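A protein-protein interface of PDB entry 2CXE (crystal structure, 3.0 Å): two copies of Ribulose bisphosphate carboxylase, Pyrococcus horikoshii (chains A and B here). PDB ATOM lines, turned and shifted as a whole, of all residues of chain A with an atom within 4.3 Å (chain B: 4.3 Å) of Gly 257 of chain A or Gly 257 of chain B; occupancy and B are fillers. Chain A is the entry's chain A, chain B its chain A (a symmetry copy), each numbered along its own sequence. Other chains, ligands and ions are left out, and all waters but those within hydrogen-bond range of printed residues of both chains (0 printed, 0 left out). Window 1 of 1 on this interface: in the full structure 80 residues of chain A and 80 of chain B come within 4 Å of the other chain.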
ATOM      1  N   ILE A 253      30.251 -12.498   5.850  1.00  0.00           N
ATOM      2  CA  ILE A 253      29.369 -13.110   4.897  1.00  0.00           C
ATOM      3  C   ILE A 253      28.066 -13.477   5.413  1.00  0.00           C
ATOM      4  O   ILE A 253      27.072 -13.185   4.633  1.00  0.00           O
ATOM      5  CB  ILE A 253      29.981 -14.141   4.071  1.00  0.00           C
ATOM      6  CG1 ILE A 253      30.233 -15.353   4.767  1.00  0.00           C
ATOM      7  CG2 ILE A 253      31.221 -13.700   3.825  1.00  0.00           C
ATOM      8  CD1 ILE A 253      31.664 -15.809   4.455  1.00  0.00           C
ATOM      9  N   VAL A 254      27.958 -13.835   6.735  1.00  0.00           N
ATOM     10  CA  VAL A 254      26.571 -14.272   7.076  1.00  0.00           C
ATOM     11  C   VAL A 254      25.435 -13.272   7.299  1.00  0.00           C
ATOM     12  O   VAL A 254      24.260 -13.501   6.832  1.00  0.00           O
ATOM     13  CB  VAL A 254      26.503 -15.398   8.139  1.00  0.00           C
ATOM     14  CG1 VAL A 254      25.214 -16.224   7.869  1.00  0.00           C
ATOM     15  CG2 VAL A 254      27.736 -16.350   8.087  1.00  0.00           C
ATOM     16  N   VAL A 255      25.967 -12.127   7.767  1.00  0.00           N
ATOM     17  CA  VAL A 255      25.389 -10.808   8.125  1.00  0.00           C
ATOM     18  C   VAL A 255      24.808 -10.004   6.935  1.00  0.00           C
ATOM     19  O   VAL A 255      23.534  -9.912   6.645  1.00  0.00           O
ATOM     20  CB  VAL A 255      26.555 -10.013   8.865  1.00  0.00           C
ATOM     21  CG1 VAL A 255      25.897  -8.923   9.799  1.00  0.00           C
ATOM     22  CG2 VAL A 255      27.559 -11.024   9.767  1.00  0.00           C
ATOM     23  N   ALA A 256      25.891  -9.660   6.224  1.00  0.00           N
ATOM     24  CA  ALA A 256      26.125  -8.999   4.944  1.00  0.00           C
ATOM     25  C   ALA A 256      25.126  -9.613   3.957  1.00  0.00           C
ATOM     26  O   ALA A 256      24.280  -8.894   3.308  1.00  0.00           O
ATOM     27  CB  ALA A 256      27.517  -9.288   4.567  1.00  0.00           C
ATOM     28  N   GLY A 257      25.147 -10.948   3.791  1.00  0.00           N
ATOM     29  CA  GLY A 257      23.990 -11.513   3.024  1.00  0.00           C
ATOM     30  C   GLY A 257      24.434 -12.223   1.786  1.00  0.00           C
ATOM     31  O   GLY A 257      25.623 -12.136   1.335  1.00  0.00           O
ATOM     32  N   TRP A 258      23.561 -12.974   1.128  1.00  0.00           N
ATOM     33  CA  TRP A 258      24.308 -13.646  -0.081  1.00  0.00           C
ATOM     34  C   TRP A 258      24.648 -12.896  -1.390  1.00  0.00           C
ATOM     35  O   TRP A 258      25.669 -12.959  -1.905  1.00  0.00           O
ATOM     36  CB  TRP A 258      23.641 -15.042  -0.511  1.00  0.00           C
ATOM     37  CG  TRP A 258      24.090 -16.328   0.296  1.00  0.00           C
ATOM     38  CD1 TRP A 258      23.296 -17.083   1.041  1.00  0.00           C
ATOM     39  CD2 TRP A 258      25.400 -16.873   0.418  1.00  0.00           C
ATOM     40  NE1 TRP A 258      23.989 -18.052   1.610  1.00  0.00           N
ATOM     41  CE2 TRP A 258      25.289 -17.980   1.256  1.00  0.00           C
ATOM     42  CE3 TRP A 258      26.646 -16.509  -0.081  1.00  0.00           C
ATOM     43  CZ2 TRP A 258      26.353 -18.817   1.626  1.00  0.00           C
ATOM     44  CZ3 TRP A 258      27.790 -17.342   0.302  1.00  0.00           C
ATOM     45  CH2 TRP A 258      27.587 -18.530   1.173  1.00  0.00           C
ATOM     46  N   SER A 259      23.640 -12.282  -1.884  1.00  0.00           N
ATOM     47  CA  SER A 259      23.580 -11.558  -3.054  1.00  0.00           C
ATOM     48  C   SER A 259      24.588 -10.415  -3.161  1.00  0.00           C
ATOM     49  O   SER A 259      25.135  -9.874  -4.188  1.00  0.00           O
ATOM     50  CB  SER A 259      22.149 -11.151  -2.960  1.00  0.00           C
ATOM     51  OG  SER A 259      22.035  -9.794  -3.236  1.00  0.00           O
ATOM     52  N   ALA A 260      24.860 -10.125  -1.953  1.00  0.00           N
ATOM     53  CA  ALA A 260      25.622  -9.063  -1.705  1.00  0.00           C
ATOM     54  C   ALA A 260      27.020  -9.490  -1.755  1.00  0.00           C
ATOM     55  O   ALA A 260      27.818  -8.812  -2.183  1.00  0.00           O
ATOM     56  CB  ALA A 260      25.150  -8.657  -0.440  1.00  0.00           C
ATOM     57  N   LEU A 261      27.298 -10.750  -1.397  1.00  0.00           N
ATOM     58  CA  LEU A 261      28.787 -11.329  -1.410  1.00  0.00           C
ATOM     59  C   LEU A 261      29.116 -11.497  -2.779  1.00  0.00           C
ATOM     60  O   LEU A 261      30.211 -11.356  -3.086  1.00  0.00           O
ATOM     61  CB  LEU A 261      29.048 -12.845  -1.009  1.00  0.00           C
ATOM     62  CG  LEU A 261      30.341 -12.928  -0.280  1.00  0.00           C
ATOM     63  CD1 LEU A 261      30.499 -14.274   0.118  1.00  0.00           C
ATOM     64  CD2 LEU A 261      31.290 -12.228  -0.820  1.00  0.00           C
ATOM     65  N   ILE B 253      14.174 -11.887   1.122  1.00  0.00           N
ATOM     66  CA  ILE B 253      15.066 -11.244   2.045  1.00  0.00           C
ATOM     67  C   ILE B 253      15.960 -12.134   2.757  1.00  0.00           C
ATOM     68  O   ILE B 253      17.185 -11.717   2.844  1.00  0.00           O
ATOM     69  CB  ILE B 253      14.446 -10.237   2.894  1.00  0.00           C
ATOM     70  CG1 ILE B 253      13.622 -10.782   3.915  1.00  0.00           C
ATOM     71  CG2 ILE B 253      13.549  -9.624   2.112  1.00  0.00           C
ATOM     72  CD1 ILE B 253      12.290 -10.021   3.929  1.00  0.00           C
ATOM     73  N   VAL B 254      15.536 -13.411   3.033  1.00  0.00           N
ATOM     74  CA  VAL B 254      16.537 -14.160   3.850  1.00  0.00           C
ATOM     75  C   VAL B 254      17.804 -14.759   3.236  1.00  0.00           C
ATOM     76  O   VAL B 254      18.930 -14.681   3.850  1.00  0.00           O
ATOM     77  CB  VAL B 254      15.915 -15.157   4.861  1.00  0.00           C
ATOM     78  CG1 VAL B 254      16.894 -15.283   6.062  1.00  0.00           C
ATOM     79  CG2 VAL B 254      14.524 -14.690   5.388  1.00  0.00           C
ATOM     80  N   VAL B 255      17.543 -15.069   1.952  1.00  0.00           N
ATOM     81  CA  VAL B 255      18.368 -15.629   0.853  1.00  0.00           C
ATOM     82  C   VAL B 255      19.511 -14.707   0.357  1.00  0.00           C
ATOM     83  O   VAL B 255      20.772 -14.837   0.684  1.00  0.00           O
ATOM     84  CB  VAL B 255      17.345 -15.986  -0.315  1.00  0.00           C
ATOM     85  CG1 VAL B 255      17.991 -17.111  -1.215  1.00  0.00           C
ATOM     86  CG2 VAL B 255      15.846 -16.495   0.267  1.00  0.00           C
ATOM     87  N   ALA B 256      18.867 -13.702  -0.251  1.00  0.00           N
ATOM     88  CA  ALA B 256      19.260 -12.433  -0.857  1.00  0.00           C
ATOM     89  C   ALA B 256      20.267 -11.794   0.106  1.00  0.00           C
ATOM     90  O   ALA B 256      21.454 -11.466  -0.267  1.00  0.00           O
ATOM     91  CB  ALA B 256      18.036 -11.627  -0.984  1.00  0.00           C
ATOM     92  N   GLY B 257      19.878 -11.591   1.379  1.00  0.00           N
ATOM     93  CA  GLY B 257      20.975 -11.213   2.328  1.00  0.00           C
ATOM     94  C   GLY B 257      20.734  -9.877   2.955  1.00  0.00           C
ATOM     95  O   GLY B 257      19.833  -9.077   2.539  1.00  0.00           O
ATOM     96  N   TRP B 258      21.482  -9.507   3.985  1.00  0.00           N
ATOM     97  CA  TRP B 258      20.974  -8.105   4.480  1.00  0.00           C
ATOM     98  C   TRP B 258      21.309  -6.778   3.760  1.00  0.00           C
ATOM     99  O   TRP B 258      20.532  -5.966   3.543  1.00  0.00           O
ATOM    100  CB  TRP B 258      21.264  -7.867   6.042  1.00  0.00           C
ATOM    101  CG  TRP B 258      20.205  -8.453   7.064  1.00  0.00           C
ATOM    102  CD1 TRP B 258      20.449  -9.388   7.970  1.00  0.00           C
ATOM    103  CD2 TRP B 258      18.821  -8.139   7.167  1.00  0.00           C
ATOM    104  NE1 TRP B 258      19.347  -9.681   8.633  1.00  0.00           N
ATOM    105  CE2 TRP B 258      18.312  -8.936   8.190  1.00  0.00           C
ATOM    106  CE3 TRP B 258      17.971  -7.283   6.475  1.00  0.00           C
ATOM    107  CZ2 TRP B 258      16.979  -8.927   8.628  1.00  0.00           C
ATOM    108  CZ3 TRP B 258      16.563  -7.261   6.884  1.00  0.00           C
ATOM    109  CH2 TRP B 258      16.102  -8.116   8.008  1.00  0.00           C
ATOM    110  N   SER B 259      22.560  -6.646   3.525  1.00  0.00           N
ATOM    111  CA  SER B 259      23.203  -5.577   2.943  1.00  0.00           C
ATOM    112  C   SER B 259      22.693  -5.190   1.556  1.00  0.00           C
ATOM    113  O   SER B 259      22.690  -4.059   0.950  1.00  0.00           O
ATOM    114  CB  SER B 259      24.587  -6.130   2.992  1.00  0.00           C
ATOM    115  OG  SER B 259      25.203  -5.943   1.760  1.00  0.00           O
ATOM    116  N   ALA B 260      22.167  -6.258   1.109  1.00  0.00           N
ATOM    117  CA  ALA B 260      21.743  -6.284  -0.152  1.00  0.00           C
ATOM    118  C   ALA B 260      20.369  -5.783  -0.174  1.00  0.00           C
ATOM    119  O   ALA B 260      19.999  -5.145  -1.033  1.00  0.00           O
ATOM    120  CB  ALA B 260      21.904  -7.644  -0.485  1.00  0.00           C
ATOM    121  N   LEU B 261      19.611  -5.997   0.908  1.00  0.00           N
ATOM    122  CA  LEU B 261      18.096  -5.498   0.999  1.00  0.00           C
ATOM    123  C   LEU B 261      18.171  -4.091   1.158  1.00  0.00           C
ATOM    124  O   LEU B 261      17.327  -3.458   0.708  1.00  0.00           O
ATOM    125  CB  LEU B 261      17.260  -5.752   2.326  1.00  0.00           C
ATOM    126  CG  LEU B 261      15.848  -6.032   1.952  1.00  0.00           C
ATOM    127  CD1 LEU B 261      15.159  -6.320   3.151  1.00  0.00           C
ATOM    128  CD2 LEU B 261      15.385  -5.241   1.036  1.00  0.00           C
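Hydrophobic or aromatic side chains of chain A within 4 Å of the printed part of chain B: Trp 258 and Ala 260. Hydrophobic or aromatic side chains of chain B within 4 Å of the printed part of chain A: Trp 258 and Ala 260. Among the printed residues, no Asp or Glu carboxylate lies within 4 Å of a Lys or Arg side-chain nitrogen of the other chain.
O of Val 255 of chain A sits close to N of Trp 258 of chain B (3.4 Å). The backbone carbonyl oxygen of Ala 256 of chain A is in hydrogen-bond range of the backbone NH of Trp 258 of chain B, 2.9 Å away. The backbone carbonyl oxygen (O) of Ala 256 of chain A sits close to the backbone NH (N) of Ser 259 of chain B (2.8 Å). The backbone carbonyl oxygen of Val 255 of chain B sits close to the backbone NH of Trp 258 of chain A (3.4 Å). The backbone carbonyl oxygen of Ala 256 of chain B is in hydrogen-bond range of the backbone NH of Trp 258 of chain A, 2.9 Å away. The backbone NH (N) of Ser 259 of chain A lies close to the backbone carbonyl oxygen (O) of Ala 256 of chain B, 2.8 Å away.
Gly 257 of chain B touches Ala 256 of chain A. Gly 257 of chain A touches Ala 256 of chain B. Gly 257 of chain B touches Gly 257 of chain A (CA to CA, 3.1 Å). Gly 257 of chain A touches Trp 258 of chain B. Trp 258 of chain A touches Gly 257 of chain B. OG of Ser 259 of chain A touches CB of Ala 260 of chain B, at 3.5 Å. Ser 259 of chain B touches Ala 260 of chain A (OG to CB, 3.5 Å). Ala 260 of chain B touches Ala 260 of chain A.
Ala 256 of chain A touches Gly 257 of chain B, and with the chains exchanged Gly 257 of chain A touches Ala 256 of chain B. Ala 256 of chain A touches Ser 259 of chain B, and with the chains exchanged Ser 259 of chain A touches Ala 256 of chain B. Gly 257 of chain A touches its own counterpart, Gly 257 of chain B. Ser 259 of chain A touches Ala 260 of chain B, and with the chains exchanged Ala 260 of chain A touches Ser 259 of chain B. Positions printed for both chains: 253, 254, 255, 256, 257, 258, 259, 260 and 261.
Gly 257 of chain A touches just these residues of chain B: Ala 256 (3.7 Å), Gly 257 (3.1 Å) and Trp 258 (3.4 Å). Gly 257 of chain B touches just these residues of chain A: Ala 256 (3.7 Å), Gly 257 (3.1 Å) and Trp 258 (3.4 Å). Of the printed residues of chain B, Val 255 of chain A touches Trp 258 (3.1 Å). Of the printed residues of chain B, Ala 256 of chain A touches Gly 257 (3.7 Å), Trp 258 (2.9 Å) and Ser 259 (2.8 Å). Printed residues of chain B within 4 Å of Trp 258 of chain A: Val 255 (3.1 Å), Ala 256 (2.9 Å) and Gly 257 (3.4 Å). Of the printed residues of chain B, Ser 259 of chain A touches Ala 256 (2.8 Å) and Ala 260 (3.5 Å). Ile 253 of chain B touches none of the printed residues of chain A. Leu 261 of chain B touches none of the printed residues of chain A. The nearest printed residue of chain A that does not touch Gly 257 of chain B is Val 255 of chain A (4.6 Å). The nearest printed residue of chain A that does not touch Ala 256 of chain B is Ala 260 of chain A (4.03 Å).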
